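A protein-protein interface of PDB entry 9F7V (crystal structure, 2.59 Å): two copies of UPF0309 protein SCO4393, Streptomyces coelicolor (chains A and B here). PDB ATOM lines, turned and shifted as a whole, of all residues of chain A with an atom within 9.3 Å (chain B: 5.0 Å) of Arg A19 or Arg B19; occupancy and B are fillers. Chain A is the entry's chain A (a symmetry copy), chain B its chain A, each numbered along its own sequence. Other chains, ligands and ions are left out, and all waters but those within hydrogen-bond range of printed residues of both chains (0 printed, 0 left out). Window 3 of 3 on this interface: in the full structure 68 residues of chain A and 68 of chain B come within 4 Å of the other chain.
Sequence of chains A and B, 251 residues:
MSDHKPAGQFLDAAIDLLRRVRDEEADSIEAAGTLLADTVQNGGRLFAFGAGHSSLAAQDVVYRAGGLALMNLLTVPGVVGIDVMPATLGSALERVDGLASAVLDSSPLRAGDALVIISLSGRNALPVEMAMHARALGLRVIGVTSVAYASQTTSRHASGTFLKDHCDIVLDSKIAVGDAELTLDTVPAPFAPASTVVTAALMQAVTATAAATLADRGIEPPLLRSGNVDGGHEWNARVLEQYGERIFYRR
The guanidinium group (NH1) of Arg B22 is in salt-bridge range of the side-chain carboxylate (OD1) of Asp A12 (2.7 Å).
NH1 of Arg B19 is in salt-bridge range of OD1 of Asp B16, at 2.6 Å. The side-chain carboxylate (OD1) of Asp B23 lies within salt-bridge range of the guanidinium group (NE) of Arg B22 (2.9 Å). The guanidinium group of Arg A19 lies within salt-bridge range of the side-chain carboxylate of Asp A16, 2.6 Å away. OD1 of Asp A23 is in salt-bridge range of NE of Arg A22, 2.9 Å away.
Leu A11 touches Arg B22 (CD1 to CA, 3.4 Å). Ile A15 touches Ile B15. Ile A15 touches Leu B18 (CG1 to CB, 3.8 Å). Ile A15 touches Arg B19 (CD1 to CG, 3.9 Å). CD1 of Ile A15 touches NH1 of Arg B22 (3.7 Å). Leu A18 touches Ile B15. Leu A18 touches Leu B18. Arg A19 touches Ile B15. Arg B19 touches Arg A19 (NH2 to NH2, 3.6 Å). CD1 of Ile B15 touches NH1 of Arg A22, at 3.7 Å.
Of chain B, only Ile B15 and Arg B19 come within 4 Å of Arg A19. Printed residues of chain A within 4 Å of Arg B19: Ile A15 (3.9 Å) and Arg A19 (3.6 Å). Arg B22 touches just these residues of chain A: Leu A11, Asp A12 and Ile A15. Printed residues of chain B within 4 Å of Leu A18: Ile B15 (3.8 Å) and Leu B18 (3.7 Å). Printed residues of chain A within 4 Å of Leu B18: Ile A15 (3.8 Å) and Leu A18 (3.7 Å). Of the printed residues of chain B, Ile A15 touches Ile B15, Leu B18, Arg B19 and Arg B22. Of the printed residues of chain B, Leu A11 touches Arg B22 (3.4 Å). Printed residues of chain B within 4 Å of Arg A22: Ile B15. The nearest printed residue of chain B that does not touch Arg A19 is Arg B22 (6.1 Å). The nearest residue of chain A that does not touch Arg B19 is Arg A22 (6.1 Å).
Hydrophobic or aromatic side chains of chain B that line the printed part of chain A: Ile B15 and Leu B18. Of the 21 printed residues of chain A, 6 touch a printed residue of chain B. Hydrophobic or aromatic side chains of chain A within 4 Å of the printed part of chain B: Leu A11, Ile A15 and Leu A18. Among the printed residues, 11 pairs touch across the chains.
Ile A15 touches its own counterpart, Ile B15. Ile A15 touches Leu B18, and with the chains exchanged Leu A18 touches Ile B15. Ile A15 touches Arg B22, and with the chains exchanged Arg A22 touches Ile B15. Arg A19 touches its own counterpart, Arg B19. 10 positions are printed for both chains. Of the 11 pairs that touch across the chains among the printed residues, 9 have their exchanged pair printed and touching as well.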
ATOM      1  N   GLY A   8      37.083 -31.015  13.739  1.00  0.00           N
ATOM      2  CA  GLY A   8      37.002 -29.643  14.215  1.00  0.00           C
ATOM      3  C   GLY A   8      37.314 -28.628  13.133  1.00  0.00           C
ATOM      4  O   GLY A   8      36.672 -27.577  13.048  1.00  0.00           O
ATOM      5  N   LEU A  11      34.146 -28.397  10.876  1.00  0.00           N
ATOM      6  CA  LEU A  11      33.057 -27.696  11.547  1.00  0.00           C
ATOM      7  C   LEU A  11      33.357 -26.207  11.681  1.00  0.00           C
ATOM      8  O   LEU A  11      32.454 -25.372  11.553  1.00  0.00           O
ATOM      9  CB  LEU A  11      32.793 -28.333  12.914  1.00  0.00           C
ATOM     10  CG  LEU A  11      32.281 -29.777  12.841  1.00  0.00           C
ATOM     11  CD1 LEU A  11      32.314 -30.444  14.206  1.00  0.00           C
ATOM     12  CD2 LEU A  11      30.875 -29.841  12.244  1.00  0.00           C
ATOM     13  N   ASP A  12      34.619 -25.850  11.932  1.00  0.00           N
ATOM     14  CA  ASP A  12      34.969 -24.433  11.985  1.00  0.00           C
ATOM     15  C   ASP A  12      34.814 -23.783  10.615  1.00  0.00           C
ATOM     16  O   ASP A  12      34.404 -22.620  10.516  1.00  0.00           O
ATOM     17  CB  ASP A  12      36.401 -24.260  12.491  1.00  0.00           C
ATOM     18  CG  ASP A  12      36.504 -24.338  14.001  1.00  0.00           C
ATOM     19  OD1 ASP A  12      35.484 -24.103  14.679  1.00  0.00           O
ATOM     20  OD2 ASP A  12      37.606 -24.642  14.507  1.00  0.00           O
ATOM     21  N   ALA A  13      35.124 -24.519   9.547  1.00  0.00           N
ATOM     22  CA  ALA A  13      34.930 -23.982   8.205  1.00  0.00           C
ATOM     23  C   ALA A  13      33.449 -23.795   7.898  1.00  0.00           C
ATOM     24  O   ALA A  13      33.053 -22.786   7.303  1.00  0.00           O
ATOM     25  CB  ALA A  13      35.578 -24.908   7.177  1.00  0.00           C
ATOM     26  N   ALA A  14      32.618 -24.756   8.299  1.00  0.00           N
ATOM     27  CA  ALA A  14      31.184 -24.650   8.058  1.00  0.00           C
ATOM     28  C   ALA A  14      30.568 -23.505   8.853  1.00  0.00           C
ATOM     29  O   ALA A  14      29.735 -22.756   8.331  1.00  0.00           O
ATOM     30  CB  ALA A  14      30.498 -25.970   8.410  1.00  0.00           C
ATOM     31  N   ILE A  15      30.963 -23.357  10.119  1.00  0.00           N
ATOM     32  CA  ILE A  15      30.525 -22.212  10.913  1.00  0.00           C
ATOM     33  C   ILE A  15      30.899 -20.904  10.226  1.00  0.00           C
ATOM     34  O   ILE A  15      30.081 -19.983  10.119  1.00  0.00           O
ATOM     35  CB  ILE A  15      31.126 -22.290  12.328  1.00  0.00           C
ATOM     36  CG1 ILE A  15      30.462 -23.417  13.124  1.00  0.00           C
ATOM     37  CG2 ILE A  15      30.968 -20.957  13.050  1.00  0.00           C
ATOM     38  CD1 ILE A  15      31.254 -23.855  14.334  1.00  0.00           C
ATOM     39  N   ASP A  16      32.140 -20.803   9.740  1.00  0.00           N
ATOM     40  CA  ASP A  16      32.582 -19.561   9.110  1.00  0.00           C
ATOM     41  C   ASP A  16      31.769 -19.259   7.858  1.00  0.00           C
ATOM     42  O   ASP A  16      31.470 -18.095   7.567  1.00  0.00           O
ATOM     43  CB  ASP A  16      34.068 -19.639   8.769  1.00  0.00           C
ATOM     44  CG  ASP A  16      34.958 -19.439   9.981  1.00  0.00           C
ATOM     45  OD1 ASP A  16      34.456 -18.968  11.025  1.00  0.00           O
ATOM     46  OD2 ASP A  16      36.165 -19.749   9.887  1.00  0.00           O
ATOM     47  N   LEU A  17      31.380 -20.298   7.117  1.00  0.00           N
ATOM     48  CA  LEU A  17      30.567 -20.083   5.929  1.00  0.00           C
ATOM     49  C   LEU A  17      29.167 -19.622   6.310  1.00  0.00           C
ATOM     50  O   LEU A  17      28.607 -18.724   5.669  1.00  0.00           O
ATOM     51  CB  LEU A  17      30.517 -21.360   5.084  1.00  0.00           C
ATOM     52  CG  LEU A  17      31.807 -21.703   4.333  1.00  0.00           C
ATOM     53  CD1 LEU A  17      31.812 -23.145   3.865  1.00  0.00           C
ATOM     54  CD2 LEU A  17      32.007 -20.766   3.143  1.00  0.00           C
ATOM     55  N   LEU A  18      28.602 -20.197   7.371  1.00  0.00           N
ATOM     56  CA  LEU A  18      27.315 -19.724   7.862  1.00  0.00           C
ATOM     57  C   LEU A  18      27.408 -18.282   8.346  1.00  0.00           C
ATOM     58  O   LEU A  18      26.472 -17.497   8.154  1.00  0.00           O
ATOM     59  CB  LEU A  18      26.816 -20.643   8.980  1.00  0.00           C
ATOM     60  CG  LEU A  18      26.469 -22.077   8.559  1.00  0.00           C
ATOM     61  CD1 LEU A  18      25.811 -22.822   9.694  1.00  0.00           C
ATOM     62  CD2 LEU A  18      25.570 -22.096   7.333  1.00  0.00           C
ATOM     63  N   ARG A  19      28.528 -17.901   8.962  1.00  0.00           N
ATOM     64  CA  ARG A  19      28.671 -16.507   9.371  1.00  0.00           C
ATOM     65  C   ARG A  19      28.710 -15.586   8.158  1.00  0.00           C
ATOM     66  O   ARG A  19      28.127 -14.496   8.177  1.00  0.00           O
ATOM     67  CB  ARG A  19      29.935 -16.304  10.206  1.00  0.00           C
ATOM     68  CG  ARG A  19      29.895 -16.875  11.611  1.00  0.00           C
ATOM     69  CD  ARG A  19      30.881 -16.127  12.507  1.00  0.00           C
ATOM     70  NE  ARG A  19      31.189 -16.843  13.741  1.00  0.00           N
ATOM     71  CZ  ARG A  19      32.266 -17.597  13.930  1.00  0.00           C
ATOM     72  NH1 ARG A  19      33.140 -17.816  12.959  1.00  0.00           N
ATOM     73  NH2 ARG A  19      32.460 -18.161  15.120  1.00  0.00           N
ATOM     74  N   ARG A  20      29.397 -16.006   7.097  1.00  0.00           N
ATOM     75  CA  ARG A  20      29.440 -15.194   5.886  1.00  0.00           C
ATOM     76  C   ARG A  20      28.049 -15.029   5.289  1.00  0.00           C
ATOM     77  O   ARG A  20      27.659 -13.923   4.897  1.00  0.00           O
ATOM     78  CB  ARG A  20      30.392 -15.829   4.876  1.00  0.00           C
ATOM     79  CG  ARG A  20      31.859 -15.612   5.196  1.00  0.00           C
ATOM     80  CD  ARG A  20      32.726 -15.884   3.986  1.00  0.00           C
ATOM     81  NE  ARG A  20      32.429 -14.959   2.900  1.00  0.00           N
ATOM     82  CZ  ARG A  20      32.806 -15.135   1.642  1.00  0.00           C
ATOM     83  NH1 ARG A  20      33.466 -16.218   1.263  1.00  0.00           N
ATOM     84  NH2 ARG A  20      32.486 -14.216   0.735  1.00  0.00           N
ATOM     85  N   VAL A  21      27.281 -16.118   5.218  1.00  0.00           N
ATOM     86  CA  VAL A  21      25.918 -16.030   4.704  1.00  0.00           C
ATOM     87  C   VAL A  21      25.083 -15.113   5.583  1.00  0.00           C
ATOM     88  O   VAL A  21      24.331 -14.265   5.088  1.00  0.00           O
ATOM     89  CB  VAL A  21      25.300 -17.437   4.607  1.00  0.00           C
ATOM     90  CG1 VAL A  21      23.792 -17.348   4.457  1.00  0.00           C
ATOM     91  CG2 VAL A  21      25.910 -18.194   3.444  1.00  0.00           C
ATOM     92  N   ARG A  22      25.209 -15.263   6.900  1.00  0.00           N
ATOM     93  CA  ARG A  22      24.442 -14.439   7.825  1.00  0.00           C
ATOM     94  C   ARG A  22      24.772 -12.966   7.647  1.00  0.00           C
ATOM     95  O   ARG A  22      23.876 -12.114   7.623  1.00  0.00           O
ATOM     96  CB  ARG A  22      24.723 -14.881   9.260  1.00  0.00           C
ATOM     97  CG  ARG A  22      23.938 -14.122  10.325  1.00  0.00           C
ATOM     98  CD  ARG A  22      24.569 -14.326  11.691  1.00  0.00           C
ATOM     99  NE  ARG A  22      25.924 -13.786  11.740  1.00  0.00           N
ATOM    100  CZ  ARG A  22      26.859 -14.178  12.594  1.00  0.00           C
ATOM    101  NH1 ARG A  22      26.598 -15.048  13.556  1.00  0.00           N
ATOM    102  NH2 ARG A  22      28.082 -13.662  12.497  1.00  0.00           N
ATOM    103  N   ASP A  23      26.062 -12.646   7.537  1.00  0.00           N
ATOM    104  CA  ASP A  23      26.498 -11.259   7.504  1.00  0.00           C
ATOM    105  C   ASP A  23      26.436 -10.631   6.116  1.00  0.00           C
ATOM    106  O   ASP A  23      26.315  -9.406   6.016  1.00  0.00           O
ATOM    107  CB  ASP A  23      27.934 -11.171   8.022  1.00  0.00           C
ATOM    108  CG  ASP A  23      28.050 -11.538   9.489  1.00  0.00           C
ATOM    109  OD1 ASP A  23      27.018 -11.528  10.192  1.00  0.00           O
ATOM    110  OD2 ASP A  23      29.175 -11.846   9.937  1.00  0.00           O
ATOM    111  N   GLU A  24      26.475 -11.427   5.047  1.00  0.00           N
ATOM    112  CA  GLU A  24      26.546 -10.888   3.692  1.00  0.00           C
ATOM    113  C   GLU A  24      25.249 -11.006   2.912  1.00  0.00           C
ATOM    114  O   GLU A  24      24.999 -10.181   2.029  1.00  0.00           O
ATOM    115  CB  GLU A  24      27.661 -11.585   2.901  1.00  0.00           C
ATOM    116  CG  GLU A  24      29.058 -11.318   3.447  1.00  0.00           C
ATOM    117  CD  GLU A  24      30.126 -12.188   2.807  1.00  0.00           C
ATOM    118  OE1 GLU A  24      29.871 -12.748   1.721  1.00  0.00           O
ATOM    119  OE2 GLU A  24      31.228 -12.302   3.383  1.00  0.00           O
ATOM    120  N   GLU A  25      24.436 -12.019   3.193  1.00  0.00           N
ATOM    121  CA  GLU A  25      23.241 -12.312   2.417  1.00  0.00           C
ATOM    122  C   GLU A  25      21.961 -11.943   3.156  1.00  0.00           C
ATOM    123  O   GLU A  25      20.872 -12.299   2.700  1.00  0.00           O
ATOM    124  CB  GLU A  25      23.226 -13.788   2.020  1.00  0.00           C
ATOM    125  CG  GLU A  25      24.464 -14.213   1.250  1.00  0.00           C
ATOM    126  CD  GLU A  25      24.640 -13.416  -0.032  1.00  0.00           C
ATOM    127  OE1 GLU A  25      23.760 -13.505  -0.914  1.00  0.00           O
ATOM    128  OE2 GLU A  25      25.651 -12.691  -0.153  1.00  0.00           O
ATOM    129  N   ALA A  26      22.063 -11.206   4.264  1.00  0.00           N
ATOM    130  CA  ALA A  26      20.875 -10.867   5.041  1.00  0.00           C
ATOM    131  C   ALA A  26      19.834 -10.148   4.191  1.00  0.00           C
ATOM    132  O   ALA A  26      18.646 -10.493   4.229  1.00  0.00           O
ATOM    133  CB  ALA A  26      21.266 -10.008   6.243  1.00  0.00           C
ATOM    134  N   ILE A  29      18.503 -12.554   1.531  1.00  0.00           N
ATOM    135  CA  ILE A  29      17.621 -13.529   2.156  1.00  0.00           C
ATOM    136  C   ILE A  29      16.275 -12.893   2.466  1.00  0.00           C
ATOM    137  O   ILE A  29      15.217 -13.497   2.247  1.00  0.00           O
ATOM    138  CB  ILE A  29      18.281 -14.097   3.426  1.00  0.00           C
ATOM    139  CG1 ILE A  29      19.474 -14.977   3.060  1.00  0.00           C
ATOM    140  CG2 ILE A  29      17.273 -14.907   4.230  1.00  0.00           C
ATOM    141  CD1 ILE A  29      20.357 -15.310   4.242  1.00  0.00           C
ATOM    142  N   LYS A 174      28.628 -18.936  -1.421  1.00  0.00           N
ATOM    143  CA  LYS A 174      29.966 -18.703  -0.876  1.00  0.00           C
ATOM    144  C   LYS A 174      31.007 -19.789  -1.150  1.00  0.00           C
ATOM    145  O   LYS A 174      32.207 -19.496  -1.152  1.00  0.00           O
ATOM    146  CB  LYS A 174      29.882 -18.512   0.643  1.00  0.00           C
ATOM    147  CG  LYS A 174      28.882 -17.468   1.130  1.00  0.00           C
ATOM    148  CD  LYS A 174      29.176 -16.072   0.598  1.00  0.00           C
ATOM    149  CE  LYS A 174      28.011 -15.134   0.862  1.00  0.00           C
ATOM    150  NZ  LYS A 174      28.195 -13.803   0.226  1.00  0.00           N
ATOM    151  N   VAL A 198      25.649 -25.404   3.994  1.00  0.00           N
ATOM    152  CA  VAL A 198      25.386 -23.989   3.739  1.00  0.00           C
ATOM    153  C   VAL A 198      24.062 -23.789   3.007  1.00  0.00           C
ATOM    154  O   VAL A 198      23.267 -22.918   3.378  1.00  0.00           O
ATOM    155  CB  VAL A 198      26.556 -23.364   2.956  1.00  0.00           C
ATOM    156  CG1 VAL A 198      26.193 -21.967   2.489  1.00  0.00           C
ATOM    157  CG2 VAL A 198      27.805 -23.330   3.816  1.00  0.00           C
ATOM    158  N   ALA A 201      20.947 -24.288   5.090  1.00  0.00           N
ATOM    159  CA  ALA A 201      20.756 -23.201   6.042  1.00  0.00           C
ATOM    160  C   ALA A 201      20.187 -21.976   5.337  1.00  0.00           C
ATOM    161  O   ALA A 201      19.289 -21.306   5.862  1.00  0.00           O
ATOM    162  CB  ALA A 201      22.077 -22.863   6.730  1.00  0.00           C
ATOM    163  N   ILE B  15      24.574 -22.181  13.835  1.00  0.00           N
ATOM    164  CA  ILE B  15      25.962 -22.056  14.273  1.00  0.00           C
ATOM    165  C   ILE B  15      26.139 -22.627  15.675  1.00  0.00           C
ATOM    166  O   ILE B  15      27.080 -23.384  15.940  1.00  0.00           O
ATOM    167  CB  ILE B  15      26.405 -20.583  14.209  1.00  0.00           C
ATOM    168  CG1 ILE B  15      26.559 -20.138  12.754  1.00  0.00           C
ATOM    169  CG2 ILE B  15      27.709 -20.384  14.974  1.00  0.00           C
ATOM    170  CD1 ILE B  15      26.561 -18.637  12.573  1.00  0.00           C
ATOM    171  N   ASP B  16      25.233 -22.281  16.593  1.00  0.00           N
ATOM    172  CA  ASP B  16      25.366 -22.755  17.969  1.00  0.00           C
ATOM    173  C   ASP B  16      25.269 -24.272  18.042  1.00  0.00           C
ATOM    174  O   ASP B  16      25.963 -24.910  18.843  1.00  0.00           O
ATOM    175  CB  ASP B  16      24.300 -22.113  18.856  1.00  0.00           C
ATOM    176  CG  ASP B  16      24.632 -20.681  19.227  1.00  0.00           C
ATOM    177  OD1 ASP B  16      25.796 -20.266  19.042  1.00  0.00           O
ATOM    178  OD2 ASP B  16      23.725 -19.970  19.710  1.00  0.00           O
ATOM    179  N   LEU B  17      24.432 -24.872  17.194  1.00  0.00           N
ATOM    180  CA  LEU B  17      24.320 -26.324  17.183  1.00  0.00           C
ATOM    181  C   LEU B  17      25.590 -26.958  16.634  1.00  0.00           C
ATOM    182  O   LEU B  17      26.065 -27.970  17.164  1.00  0.00           O
ATOM    183  CB  LEU B  17      23.094 -26.754  16.373  1.00  0.00           C
ATOM    184  CG  LEU B  17      21.739 -26.495  17.041  1.00  0.00           C
ATOM    185  CD1 LEU B  17      20.602 -26.568  16.041  1.00  0.00           C
ATOM    186  CD2 LEU B  17      21.500 -27.486  18.178  1.00  0.00           C
ATOM    187  N   LEU B  18      26.174 -26.358  15.597  1.00  0.00           N
ATOM    188  CA  LEU B  18      27.453 -26.842  15.095  1.00  0.00           C
ATOM    189  C   LEU B  18      28.546 -26.699  16.148  1.00  0.00           C
ATOM    190  O   LEU B  18      29.421 -27.565  16.261  1.00  0.00           O
ATOM    191  CB  LEU B  18      27.828 -26.089  13.816  1.00  0.00           C
ATOM    192  CG  LEU B  18      26.916 -26.337  12.607  1.00  0.00           C
ATOM    193  CD1 LEU B  18      27.493 -25.701  11.366  1.00  0.00           C
ATOM    194  CD2 LEU B  18      26.690 -27.822  12.373  1.00  0.00           C
ATOM    195  N   ARG B  19      28.512 -25.627  16.941  1.00  0.00           N
ATOM    196  CA  ARG B  19      29.505 -25.503  18.004  1.00  0.00           C
ATOM    197  C   ARG B  19      29.331 -26.605  19.041  1.00  0.00           C
ATOM    198  O   ARG B  19      30.316 -27.157  19.545  1.00  0.00           O
ATOM    199  CB  ARG B  19      29.413 -24.139  18.689  1.00  0.00           C
ATOM    200  CG  ARG B  19      29.909 -22.959  17.874  1.00  0.00           C
ATOM    201  CD  ARG B  19      30.332 -21.823  18.805  1.00  0.00           C
ATOM    202  NE  ARG B  19      30.449 -20.538  18.123  1.00  0.00           N
ATOM    203  CZ  ARG B  19      29.513 -19.597  18.115  1.00  0.00           C
ATOM    204  NH1 ARG B  19      28.336 -19.783  18.694  1.00  0.00           N
ATOM    205  NH2 ARG B  19      29.758 -18.445  17.496  1.00  0.00           N
ATOM    206  N   ARG B  20      28.084 -26.933  19.378  1.00  0.00           N
ATOM    207  CA  ARG B  20      27.844 -28.009  20.332  1.00  0.00           C
ATOM    208  C   ARG B  20      28.364 -29.337  19.801  1.00  0.00           C
ATOM    209  O   ARG B  20      29.014 -30.096  20.530  1.00  0.00           O
ATOM    210  CB  ARG B  20      26.352 -28.096  20.642  1.00  0.00           C
ATOM    211  CG  ARG B  20      25.857 -27.014  21.582  1.00  0.00           C
ATOM    212  CD  ARG B  20      24.513 -27.379  22.174  1.00  0.00           C
ATOM    213  NE  ARG B  20      24.600 -28.583  22.989  1.00  0.00           N
ATOM    214  CZ  ARG B  20      23.557 -29.300  23.382  1.00  0.00           C
ATOM    215  NH1 ARG B  20      22.324 -28.981  23.019  1.00  0.00           N
ATOM    216  NH2 ARG B  20      23.758 -30.378  24.134  1.00  0.00           N
ATOM    217  N   VAL B  21      28.095 -29.634  18.529  1.00  0.00           N
ATOM    218  CA  VAL B  21      28.603 -30.866  17.932  1.00  0.00           C
ATOM    219  C   VAL B  21      30.123 -30.868  17.942  1.00  0.00           C
ATOM    220  O   VAL B  21      30.759 -31.872  18.286  1.00  0.00           O
ATOM    221  CB  VAL B  21      28.046 -31.030  16.507  1.00  0.00           C
ATOM    222  CG1 VAL B  21      28.846 -32.067  15.738  1.00  0.00           C
ATOM    223  CG2 VAL B  21      26.582 -31.416  16.561  1.00  0.00           C
ATOM    224  N   ARG B  22      30.728 -29.740  17.572  1.00  0.00           N
ATOM    225  CA  ARG B  22      32.181 -29.646  17.537  1.00  0.00           C
ATOM    226  C   ARG B  22      32.777 -29.882  18.916  1.00  0.00           C
ATOM    227  O   ARG B  22      33.769 -30.607  19.063  1.00  0.00           O
ATOM    228  CB  ARG B  22      32.595 -28.276  17.003  1.00  0.00           C
ATOM    229  CG  ARG B  22      34.100 -28.072  16.871  1.00  0.00           C
ATOM    230  CD  ARG B  22      34.422 -26.594  16.741  1.00  0.00           C
ATOM    231  NE  ARG B  22      34.026 -25.853  17.934  1.00  0.00           N
ATOM    232  CZ  ARG B  22      33.770 -24.552  17.962  1.00  0.00           C
ATOM    233  NH1 ARG B  22      33.952 -23.788  16.897  1.00  0.00           N
ATOM    234  NH2 ARG B  22      33.347 -23.999  19.095  1.00  0.00           N
ATOM    235  N   ASP B  23      32.192 -29.259  19.940  1.00  0.00           N
ATOM    236  CA  ASP B  23      32.763 -29.302  21.277  1.00  0.00           C
ATOM    237  C   ASP B  23      32.367 -30.541  22.072  1.00  0.00           C
ATOM    238  O   ASP B  23      33.109 -30.935  22.977  1.00  0.00           O
ATOM    239  CB  ASP B  23      32.322 -28.058  22.050  1.00  0.00           C
ATOM    240  CG  ASP B  23      32.891 -26.777  21.469  1.00  0.00           C
ATOM    241  OD1 ASP B  23      33.874 -26.851  20.705  1.00  0.00           O
ATOM    242  OD2 ASP B  23      32.345 -25.695  21.772  1.00  0.00           O
ATOM    243  N   GLU B  24      31.249 -31.188  21.742  1.00  0.00           N
ATOM    244  CA  GLU B  24      30.746 -32.304  22.537  1.00  0.00           C
ATOM    245  C   GLU B  24      30.939 -33.662  21.886  1.00  0.00           C
ATOM    246  O   GLU B  24      31.058 -34.661  22.600  1.00  0.00           O
ATOM    247  CB  GLU B  24      29.254 -32.111  22.839  1.00  0.00           C
ATOM    248  CG  GLU B  24      28.959 -30.904  23.722  1.00  0.00           C
ATOM    249  CD  GLU B  24      27.477 -30.589  23.825  1.00  0.00           C
ATOM    250  OE1 GLU B  24      26.651 -31.472  23.512  1.00  0.00           O
ATOM    251  OE2 GLU B  24      27.135 -29.459  24.234  1.00  0.00           O
